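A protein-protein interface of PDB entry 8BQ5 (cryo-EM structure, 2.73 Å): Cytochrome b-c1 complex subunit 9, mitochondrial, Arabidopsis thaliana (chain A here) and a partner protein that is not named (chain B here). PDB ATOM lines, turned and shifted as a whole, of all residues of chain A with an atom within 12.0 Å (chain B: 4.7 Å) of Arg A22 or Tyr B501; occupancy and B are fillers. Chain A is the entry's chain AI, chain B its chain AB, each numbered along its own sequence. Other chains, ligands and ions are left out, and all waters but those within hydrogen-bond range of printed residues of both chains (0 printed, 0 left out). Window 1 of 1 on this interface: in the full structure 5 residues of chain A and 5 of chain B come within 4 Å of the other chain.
OD1 of Asn B497 sits at hydrogen-bond distance from NH1 of Arg A22 (2.4 Å).
The side-chain carboxylate (OD2) of Asp B502 lies within hydrogen-bond range of the side-chain hydroxyl (OH) of Tyr A17, 2.4 Å away.
O of Arg A22 lies within hydrogen-bond range of OH of Tyr B501.
Printed residues of chain A within 4 Å of Tyr B501: Tyr A17, Met A21 and Arg A22.
No residue of chain A comes within 4 Å of Ala B431.
Of chain A, only Tyr A17 comes within 4 Å of Asp B502.
No residue of chain A comes within 4 Å of Lys B503.
Thr B526 touches none of the printed residues of chain A.
Printed residues of chain B within 4 Å of Met A21: Tyr B501.
Of the printed residues of chain B, Tyr A17 touches Tyr B501 and Asp B502.
The nearest printed residue of chain B that does not touch Arg A22 is Tyr B432 (5.6 Å).
The nearest residue of chain A that does not touch Tyr B501 is Arg A23 (4.5 Å).
The nearest printed residue of chain B that does not touch Met A21 is Asp B502 (5.4 Å).
The backbone NH of Tyr B501 lies within hydrogen-bond range of the backbone carbonyl oxygen of Ala B496, 3.1 Å away.
O of Tyr A17 lies within hydrogen-bond range of N of Arg A22.
The backbone NH of Asp B502 sits at hydrogen-bond distance from the backbone carbonyl oxygen of Thr B526, at 3.2 Å.
The backbone carbonyl oxygen (O) of Ala B431 is in hydrogen-bond range of the side-chain amide nitrogen (ND2) of Asn B497.
OH of Tyr A17 touches CE2 of Tyr B501, 3.96 Å away.
O of Met A21 touches OH of Tyr B501 (3.9 Å).
Of the 19 printed residues of chain A, 3 touch a printed residue of chain B.
Hydrophobic or aromatic side chains of chain B that line the printed part of chain A: Tyr B501.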
ATOM      1  N   PHE A  13      -2.869  11.264   6.074  1.00  0.00           N
ATOM      2  CA  PHE A  13      -2.945  12.154   7.226  1.00  0.00           C
ATOM      3  C   PHE A  13      -1.558  12.618   7.655  1.00  0.00           C
ATOM      4  O   PHE A  13      -1.403  13.251   8.698  1.00  0.00           O
ATOM      5  CB  PHE A  13      -3.648  11.461   8.394  1.00  0.00           C
ATOM      6  CG  PHE A  13      -5.130  11.322   8.211  1.00  0.00           C
ATOM      7  CD1 PHE A  13      -5.652  10.318   7.413  1.00  0.00           C
ATOM      8  CD2 PHE A  13      -6.003  12.194   8.837  1.00  0.00           C
ATOM      9  CE1 PHE A  13      -7.012  10.189   7.241  1.00  0.00           C
ATOM     10  CE2 PHE A  13      -7.368  12.069   8.668  1.00  0.00           C
ATOM     11  CZ  PHE A  13      -7.872  11.064   7.869  1.00  0.00           C
ATOM     12  N   GLU A  14      -0.551  12.300   6.839  1.00  0.00           N
ATOM     13  CA  GLU A  14       0.824  12.628   7.198  1.00  0.00           C
ATOM     14  C   GLU A  14       1.078  14.130   7.174  1.00  0.00           C
ATOM     15  O   GLU A  14       1.931  14.622   7.921  1.00  0.00           O
ATOM     16  CB  GLU A  14       1.796  11.908   6.264  1.00  0.00           C
ATOM     17  CG  GLU A  14       1.898  10.411   6.512  1.00  0.00           C
ATOM     18  CD  GLU A  14       2.665  10.078   7.778  1.00  0.00           C
ATOM     19  OE1 GLU A  14       2.294   9.102   8.461  1.00  0.00           O
ATOM     20  OE2 GLU A  14       3.641  10.792   8.090  1.00  0.00           O
ATOM     21  N   GLY A  15       0.367  14.871   6.322  1.00  0.00           N
ATOM     22  CA  GLY A  15       0.490  16.319   6.348  1.00  0.00           C
ATOM     23  C   GLY A  15      -0.012  16.910   7.651  1.00  0.00           C
ATOM     24  O   GLY A  15       0.631  17.782   8.244  1.00  0.00           O
ATOM     25  N   PHE A  16      -1.170  16.439   8.117  1.00  0.00           N
ATOM     26  CA  PHE A  16      -1.671  16.852   9.423  1.00  0.00           C
ATOM     27  C   PHE A  16      -0.794  16.321  10.548  1.00  0.00           C
ATOM     28  O   PHE A  16      -0.642  16.983  11.581  1.00  0.00           O
ATOM     29  CB  PHE A  16      -3.115  16.380   9.594  1.00  0.00           C
ATOM     30  CG  PHE A  16      -3.755  16.827  10.875  1.00  0.00           C
ATOM     31  CD1 PHE A  16      -3.882  15.955  11.942  1.00  0.00           C
ATOM     32  CD2 PHE A  16      -4.238  18.119  11.011  1.00  0.00           C
ATOM     33  CE1 PHE A  16      -4.473  16.361  13.122  1.00  0.00           C
ATOM     34  CE2 PHE A  16      -4.832  18.530  12.189  1.00  0.00           C
ATOM     35  CZ  PHE A  16      -4.948  17.650  13.245  1.00  0.00           C
ATOM     36  N   TYR A  17      -0.213  15.133  10.366  1.00  0.00           N
ATOM     37  CA  TYR A  17       0.674  14.564  11.376  1.00  0.00           C
ATOM     38  C   TYR A  17       1.883  15.457  11.615  1.00  0.00           C
ATOM     39  O   TYR A  17       2.288  15.684  12.761  1.00  0.00           O
ATOM     40  CB  TYR A  17       1.121  13.165  10.945  1.00  0.00           C
ATOM     41  CG  TYR A  17       2.159  12.546  11.852  1.00  0.00           C
ATOM     42  CD1 TYR A  17       1.784  11.819  12.971  1.00  0.00           C
ATOM     43  CD2 TYR A  17       3.518  12.692  11.593  1.00  0.00           C
ATOM     44  CE1 TYR A  17       2.727  11.259  13.807  1.00  0.00           C
ATOM     45  CE2 TYR A  17       4.466  12.136  12.423  1.00  0.00           C
ATOM     46  CZ  TYR A  17       4.064  11.420  13.529  1.00  0.00           C
ATOM     47  OH  TYR A  17       5.005  10.860  14.359  1.00  0.00           O
ATOM     48  N   LYS A  18       2.477  15.971  10.536  1.00  0.00           N
ATOM     49  CA  LYS A  18       3.703  16.752  10.643  1.00  0.00           C
ATOM     50  C   LYS A  18       3.492  18.070  11.379  1.00  0.00           C
ATOM     51  O   LYS A  18       4.461  18.667  11.857  1.00  0.00           O
ATOM     52  CB  LYS A  18       4.265  17.007   9.240  1.00  0.00           C
ATOM     53  CG  LYS A  18       5.574  17.777   9.192  1.00  0.00           C
ATOM     54  CD  LYS A  18       6.130  17.834   7.779  1.00  0.00           C
ATOM     55  CE  LYS A  18       5.276  18.713   6.880  1.00  0.00           C
ATOM     56  NZ  LYS A  18       4.356  17.909   6.027  1.00  0.00           N
ATOM     57  N   LEU A  19       2.248  18.529  11.499  1.00  0.00           N
ATOM     58  CA  LEU A  19       1.966  19.812  12.126  1.00  0.00           C
ATOM     59  C   LEU A  19       1.470  19.688  13.561  1.00  0.00           C
ATOM     60  O   LEU A  19       1.845  20.502  14.409  1.00  0.00           O
ATOM     61  CB  LEU A  19       0.938  20.587  11.297  1.00  0.00           C
ATOM     62  CG  LEU A  19       1.042  22.111  11.371  1.00  0.00           C
ATOM     63  CD1 LEU A  19       2.043  22.627  10.351  1.00  0.00           C
ATOM     64  CD2 LEU A  19      -0.319  22.751  11.163  1.00  0.00           C
ATOM     65  N   ILE A  20       0.631  18.695  13.857  1.00  0.00           N
ATOM     66  CA  ILE A  20       0.028  18.579  15.175  1.00  0.00           C
ATOM     67  C   ILE A  20       0.681  17.488  16.024  1.00  0.00           C
ATOM     68  O   ILE A  20       0.976  17.733  17.199  1.00  0.00           O
ATOM     69  CB  ILE A  20      -1.500  18.352  15.082  1.00  0.00           C
ATOM     70  CG1 ILE A  20      -2.283  19.650  14.819  1.00  0.00           C
ATOM     71  CG2 ILE A  20      -2.033  17.774  16.376  1.00  0.00           C
ATOM     72  CD1 ILE A  20      -1.769  20.558  13.729  1.00  0.00           C
ATOM     73  N   MET A  21       0.928  16.302  15.468  1.00  0.00           N
ATOM     74  CA  MET A  21       1.401  15.160  16.242  1.00  0.00           C
ATOM     75  C   MET A  21       2.896  15.193  16.536  1.00  0.00           C
ATOM     76  O   MET A  21       3.373  14.364  17.315  1.00  0.00           O
ATOM     77  CB  MET A  21       1.082  13.851  15.515  1.00  0.00           C
ATOM     78  CG  MET A  21      -0.388  13.531  15.302  1.00  0.00           C
ATOM     79  SD  MET A  21      -1.316  13.278  16.819  1.00  0.00           S
ATOM     80  CE  MET A  21      -2.949  12.936  16.164  1.00  0.00           C
ATOM     81  N   ARG A  22       3.648  16.116  15.928  1.00  0.00           N
ATOM     82  CA  ARG A  22       5.103  16.087  16.058  1.00  0.00           C
ATOM     83  C   ARG A  22       5.552  16.258  17.504  1.00  0.00           C
ATOM     84  O   ARG A  22       6.466  15.560  17.955  1.00  0.00           O
ATOM     85  CB  ARG A  22       5.731  17.172  15.186  1.00  0.00           C
ATOM     86  CG  ARG A  22       6.063  16.724  13.779  1.00  0.00           C
ATOM     87  CD  ARG A  22       6.949  15.496  13.780  1.00  0.00           C
ATOM     88  NE  ARG A  22       8.342  15.834  14.038  1.00  0.00           N
ATOM     89  CZ  ARG A  22       9.354  14.992  13.896  1.00  0.00           C
ATOM     90  NH1 ARG A  22      10.590  15.339  14.209  1.00  0.00           N
ATOM     91  NH2 ARG A  22       9.121  13.773  13.417  1.00  0.00           N
ATOM     92  N   ARG A  23       4.932  17.177  18.236  1.00  0.00           N
ATOM     93  CA  ARG A  23       5.233  17.410  19.639  1.00  0.00           C
ATOM     94  C   ARG A  23       4.003  17.092  20.474  1.00  0.00           C
ATOM     95  O   ARG A  23       2.874  17.373  20.061  1.00  0.00           O
ATOM     96  CB  ARG A  23       5.669  18.857  19.881  1.00  0.00           C
ATOM     97  CG  ARG A  23       6.910  19.266  19.112  1.00  0.00           C
ATOM     98  CD  ARG A  23       8.145  18.605  19.695  1.00  0.00           C
ATOM     99  NE  ARG A  23       9.359  19.016  19.004  1.00  0.00           N
ATOM    100  CZ  ARG A  23       9.888  18.372  17.973  1.00  0.00           C
ATOM    101  NH1 ARG A  23       9.329  17.277  17.482  1.00  0.00           N
ATOM    102  NH2 ARG A  23      11.003  18.838  17.419  1.00  0.00           N
ATOM    103  N   ASN A  24       4.224  16.495  21.645  1.00  0.00           N
ATOM    104  CA  ASN A  24       3.100  16.172  22.514  1.00  0.00           C
ATOM    105  C   ASN A  24       2.459  17.424  23.097  1.00  0.00           C
ATOM    106  O   ASN A  24       1.266  17.412  23.422  1.00  0.00           O
ATOM    107  CB  ASN A  24       3.545  15.233  23.632  1.00  0.00           C
ATOM    108  CG  ASN A  24       2.385  14.491  24.259  1.00  0.00           C
ATOM    109  OD1 ASN A  24       1.542  13.934  23.557  1.00  0.00           O
ATOM    110  ND2 ASN A  24       2.335  14.481  25.585  1.00  0.00           N
ATOM    111  N   SER A  25       3.228  18.504  23.246  1.00  0.00           N
ATOM    112  CA  SER A  25       2.657  19.756  23.734  1.00  0.00           C
ATOM    113  C   SER A  25       1.639  20.310  22.746  1.00  0.00           C
ATOM    114  O   SER A  25       0.582  20.815  23.140  1.00  0.00           O
ATOM    115  CB  SER A  25       3.768  20.772  23.996  1.00  0.00           C
ATOM    116  OG  SER A  25       4.790  20.667  23.021  1.00  0.00           O
ATOM    117  N   VAL A  26       1.949  20.232  21.451  1.00  0.00           N
ATOM    118  CA  VAL A  26       1.000  20.664  20.430  1.00  0.00           C
ATOM    119  C   VAL A  26      -0.175  19.697  20.353  1.00  0.00           C
ATOM    120  O   VAL A  26      -1.328  20.109  20.183  1.00  0.00           O
ATOM    121  CB  VAL A  26       1.710  20.807  19.071  1.00  0.00           C
ATOM    122  CG1 VAL A  26       0.731  21.264  18.005  1.00  0.00           C
ATOM    123  CG2 VAL A  26       2.870  21.779  19.186  1.00  0.00           C
ATOM    124  N   TYR A  27       0.101  18.396  20.473  1.00  0.00           N
ATOM    125  CA  TYR A  27      -0.965  17.400  20.418  1.00  0.00           C
ATOM    126  C   TYR A  27      -1.938  17.566  21.579  1.00  0.00           C
ATOM    127  O   TYR A  27      -3.155  17.440  21.401  1.00  0.00           O
ATOM    128  CB  TYR A  27      -0.366  15.993  20.419  1.00  0.00           C
ATOM    129  CG  TYR A  27      -1.376  14.892  20.199  1.00  0.00           C
ATOM    130  CD1 TYR A  27      -2.178  14.873  19.067  1.00  0.00           C
ATOM    131  CD2 TYR A  27      -1.530  13.872  21.128  1.00  0.00           C
ATOM    132  CE1 TYR A  27      -3.102  13.868  18.863  1.00  0.00           C
ATOM    133  CE2 TYR A  27      -2.451  12.863  20.932  1.00  0.00           C
ATOM    134  CZ  TYR A  27      -3.234  12.866  19.800  1.00  0.00           C
ATOM    135  OH  TYR A  27      -4.152  11.862  19.604  1.00  0.00           O
ATOM    136  N   VAL A  28      -1.419  17.840  22.776  1.00  0.00           N
ATOM    137  CA  VAL A  28      -2.282  18.053  23.935  1.00  0.00           C
ATOM    138  C   VAL A  28      -3.133  19.303  23.741  1.00  0.00           C
ATOM    139  O   VAL A  28      -4.328  19.314  24.059  1.00  0.00           O
ATOM    140  CB  VAL A  28      -1.435  18.125  25.218  1.00  0.00           C
ATOM    141  CG1 VAL A  28      -2.156  18.912  26.301  1.00  0.00           C
ATOM    142  CG2 VAL A  28      -1.092  16.726  25.704  1.00  0.00           C
ATOM    143  N   THR A  29      -2.534  20.372  23.210  1.00  0.00           N
ATOM    144  CA  THR A  29      -3.289  21.589  22.929  1.00  0.00           C
ATOM    145  C   THR A  29      -4.352  21.344  21.865  1.00  0.00           C
ATOM    146  O   THR A  29      -5.450  21.909  21.930  1.00  0.00           O
ATOM    147  CB  THR A  29      -2.337  22.703  22.496  1.00  0.00           C
ATOM    148  OG1 THR A  29      -1.267  22.812  23.443  1.00  0.00           O
ATOM    149  CG2 THR A  29      -3.067  24.034  22.416  1.00  0.00           C
ATOM    150  N   PHE A  30      -4.040  20.508  20.872  1.00  0.00           N
ATOM    151  CA  PHE A  30      -5.023  20.156  19.851  1.00  0.00           C
ATOM    152  C   PHE A  30      -6.208  19.417  20.460  1.00  0.00           C
ATOM    153  O   PHE A  30      -7.361  19.662  20.086  1.00  0.00           O
ATOM    154  CB  PHE A  30      -4.352  19.319  18.759  1.00  0.00           C
ATOM    155  CG  PHE A  30      -5.312  18.630  17.830  1.00  0.00           C
ATOM    156  CD1 PHE A  30      -6.052  19.352  16.910  1.00  0.00           C
ATOM    157  CD2 PHE A  30      -5.452  17.251  17.857  1.00  0.00           C
ATOM    158  CE1 PHE A  30      -6.927  18.716  16.050  1.00  0.00           C
ATOM    159  CE2 PHE A  30      -6.324  16.610  16.998  1.00  0.00           C
ATOM    160  CZ  PHE A  30      -7.062  17.344  16.094  1.00  0.00           C
ATOM    161  N   ILE A  31      -5.944  18.508  21.400  1.00  0.00           N
ATOM    162  CA  ILE A  31      -7.025  17.781  22.063  1.00  0.00           C
ATOM    163  C   ILE A  31      -7.880  18.731  22.891  1.00  0.00           C
ATOM    164  O   ILE A  31      -9.113  18.618  22.919  1.00  0.00           O
ATOM    165  CB  ILE A  31      -6.451  16.633  22.915  1.00  0.00           C
ATOM    166  CG1 ILE A  31      -5.984  15.489  22.014  1.00  0.00           C
ATOM    167  CG2 ILE A  31      -7.480  16.129  23.913  1.00  0.00           C
ATOM    168  CD1 ILE A  31      -5.084  14.498  22.709  1.00  0.00           C
ATOM    169  N   ALA B 431      17.121  12.345  18.830  1.00  0.00           N
ATOM    170  CA  ALA B 431      16.191  13.271  18.200  1.00  0.00           C
ATOM    171  C   ALA B 431      15.874  14.481  19.068  1.00  0.00           C
ATOM    172  O   ALA B 431      15.213  15.407  18.588  1.00  0.00           O
ATOM    173  CB  ALA B 431      14.892  12.547  17.840  1.00  0.00           C
ATOM    174  N   TYR B 432      16.320  14.499  20.322  1.00  0.00           N
ATOM    175  CA  TYR B 432      16.002  15.587  21.239  1.00  0.00           C
ATOM    176  C   TYR B 432      17.225  16.371  21.682  1.00  0.00           C
ATOM    177  O   TYR B 432      17.270  17.592  21.500  1.00  0.00           O
ATOM    178  CB  TYR B 432      15.272  15.031  22.469  1.00  0.00           C
ATOM    179  CG  TYR B 432      13.901  14.476  22.170  1.00  0.00           C
ATOM    180  CD1 TYR B 432      12.814  15.318  22.000  1.00  0.00           C
ATOM    181  CD2 TYR B 432      13.698  13.108  22.054  1.00  0.00           C
ATOM    182  CE1 TYR B 432      11.561  14.814  21.729  1.00  0.00           C
ATOM    183  CE2 TYR B 432      12.450  12.596  21.783  1.00  0.00           C
ATOM    184  CZ  TYR B 432      11.385  13.453  21.622  1.00  0.00           C
ATOM    185  OH  TYR B 432      10.138  12.945  21.353  1.00  0.00           O
ATOM    186  N   ALA B 496      17.934  11.971  12.923  1.00  0.00           N
ATOM    187  CA  ALA B 496      17.287  11.105  13.903  1.00  0.00           C
ATOM    188  C   ALA B 496      15.777  11.305  13.902  1.00  0.00           C
ATOM    189  O   ALA B 496      15.015  10.350  14.085  1.00  0.00           O
ATOM    190  CB  ALA B 496      17.860  11.360  15.296  1.00  0.00           C
ATOM    191  N   ASN B 497      15.327  12.544  13.704  1.00  0.00           N
ATOM    192  CA  ASN B 497      13.895  12.813  13.642  1.00  0.00           C
ATOM    193  C   ASN B 497      13.260  12.186  12.409  1.00  0.00           C
ATOM    194  O   ASN B 497      12.048  11.947  12.390  1.00  0.00           O
ATOM    195  CB  ASN B 497      13.655  14.320  13.657  1.00  0.00           C
ATOM    196  CG  ASN B 497      13.499  14.868  15.059  1.00  0.00           C
ATOM    197  OD1 ASN B 497      12.439  14.750  15.670  1.00  0.00           O
ATOM    198  ND2 ASN B 497      14.562  15.468  15.580  1.00  0.00           N
ATOM    199  N   TYR B 499      14.462   9.203  10.857  1.00  0.00           N
ATOM    200  CA  TYR B 499      14.607   7.753  10.845  1.00  0.00           C
ATOM    201  C   TYR B 499      14.202   7.073  12.140  1.00  0.00           C
ATOM    202  O   TYR B 499      13.804   5.908  12.106  1.00  0.00           O
ATOM    203  CB  TYR B 499      16.060   7.371  10.535  1.00  0.00           C
ATOM    204  CG  TYR B 499      16.477   7.640   9.111  1.00  0.00           C
ATOM    205  CD1 TYR B 499      16.117   6.776   8.089  1.00  0.00           C
ATOM    206  CD2 TYR B 499      17.230   8.759   8.791  1.00  0.00           C
ATOM    207  CE1 TYR B 499      16.498   7.017   6.787  1.00  0.00           C
ATOM    208  CE2 TYR B 499      17.615   9.009   7.492  1.00  0.00           C
ATOM    209  CZ  TYR B 499      17.246   8.134   6.494  1.00  0.00           C
ATOM    210  OH  TYR B 499      17.625   8.378   5.196  1.00  0.00           O
ATOM    211  N   ILE B 500      14.292   7.757  13.274  1.00  0.00           N
ATOM    212  CA  ILE B 500      14.127   7.141  14.584  1.00  0.00           C
ATOM    213  C   ILE B 500      12.820   7.566  15.245  1.00  0.00           C
ATOM    214  O   ILE B 500      12.090   6.734  15.785  1.00  0.00           O
ATOM    215  CB  ILE B 500      15.337   7.453  15.494  1.00  0.00           C
ATOM    216  CG1 ILE B 500      16.531   6.582  15.105  1.00  0.00           C
ATOM    217  CG2 ILE B 500      14.981   7.250  16.957  1.00  0.00           C
ATOM    218  CD1 ILE B 500      17.857   7.293  15.201  1.00  0.00           C
ATOM    219  N   TYR B 501      12.507   8.859  15.205  1.00  0.00           N
ATOM    220  CA  TYR B 501      11.393   9.377  15.989  1.00  0.00           C
ATOM    221  C   TYR B 501      10.064   8.821  15.495  1.00  0.00           C
ATOM    222  O   TYR B 501       9.704   8.985  14.326  1.00  0.00           O
ATOM    223  CB  TYR B 501      11.374  10.905  15.937  1.00  0.00           C
ATOM    224  CG  TYR B 501      10.172  11.508  16.623  1.00  0.00           C
ATOM    225  CD1 TYR B 501      10.164  11.716  17.994  1.00  0.00           C
ATOM    226  CD2 TYR B 501       9.039  11.862  15.902  1.00  0.00           C
ATOM    227  CE1 TYR B 501       9.067  12.261  18.624  1.00  0.00           C
ATOM    228  CE2 TYR B 501       7.938  12.407  16.525  1.00  0.00           C
ATOM    229  CZ  TYR B 501       7.957  12.604  17.887  1.00  0.00           C
ATOM    230  OH  TYR B 501       6.862  13.147  18.514  1.00  0.00           O
ATOM    231  N   ASP B 502       9.332   8.176  16.404  1.00  0.00           N
ATOM    232  CA  ASP B 502       7.983   7.678  16.141  1.00  0.00           C
ATOM    233  C   ASP B 502       7.948   6.798  14.894  1.00  0.00           C
ATOM    234  O   ASP B 502       7.081   6.932  14.028  1.00  0.00           O
ATOM    235  CB  ASP B 502       6.995   8.837  16.018  1.00  0.00           C
ATOM    236  CG  ASP B 502       5.575   8.422  16.327  1.00  0.00           C
ATOM    237  OD1 ASP B 502       5.370   7.266  16.747  1.00  0.00           O
ATOM    238  OD2 ASP B 502       4.662   9.252  16.139  1.00  0.00           O
ATOM    239  N   LYS B 503       8.909   5.887  14.806  1.00  0.00           N
ATOM    240  CA  LYS B 503       9.049   5.017  13.653  1.00  0.00           C
ATOM    241  C   LYS B 503       8.903   3.562  14.074  1.00  0.00           C
ATOM    242  O   LYS B 503       9.241   3.186  15.200  1.00  0.00           O
ATOM    243  CB  LYS B 503      10.399   5.228  12.961  1.00  0.00           C
ATOM    244  CG  LYS B 503      10.401   6.374  11.969  1.00  0.00           C
ATOM    245  CD  LYS B 503       9.333   6.173  10.910  1.00  0.00           C
ATOM    246  CE  LYS B 503       9.336   7.304   9.901  1.00  0.00           C
ATOM    247  NZ  LYS B 503      10.706   7.834   9.671  1.00  0.00           N
ATOM    248  N   THR B 526       9.918   5.025  21.260  1.00  0.00           N
ATOM    249  CA  THR B 526      10.543   5.745  20.160  1.00  0.00           C
ATOM    250  C   THR B 526      10.262   7.242  20.192  1.00  0.00           C
ATOM    251  O   THR B 526      10.727   7.962  19.304  1.00  0.00           O
ATOM    252  CB  THR B 526      10.078   5.176  18.815  1.00  0.00           C
ATOM    253  OG1 THR B 526       8.649   5.098  18.794  1.00  0.00           O
ATOM    254  CG2 THR B 526      10.659   3.794  18.592  1.00  0.00           C
ATOM    255  N   TYR B 527       9.515   7.721  21.184  1.00  0.00           N
ATOM    256  CA  TYR B 527       9.238   9.141  21.336  1.00  0.00           C
ATOM    257  C   TYR B 527       9.110   9.460  22.818  1.00  0.00           C
ATOM    258  O   TYR B 527       8.884   8.578  23.650  1.00  0.00           O
ATOM    259  CB  TYR B 527       7.969   9.558  20.580  1.00  0.00           C
ATOM    260  CG  TYR B 527       6.754   8.709  20.876  1.00  0.00           C
ATOM    261  CD1 TYR B 527       6.479   7.572  20.129  1.00  0.00           C
ATOM    262  CD2 TYR B 527       5.881   9.046  21.900  1.00  0.00           C
ATOM    263  CE1 TYR B 527       5.373   6.794  20.396  1.00  0.00           C
ATOM    264  CE2 TYR B 527       4.772   8.273  22.175  1.00  0.00           C
ATOM    265  CZ  TYR B 527       4.523   7.149  21.419  1.00  0.00           C
ATOM    266  OH  TYR B 527       3.418   6.378  21.688  1.00  0.00           O
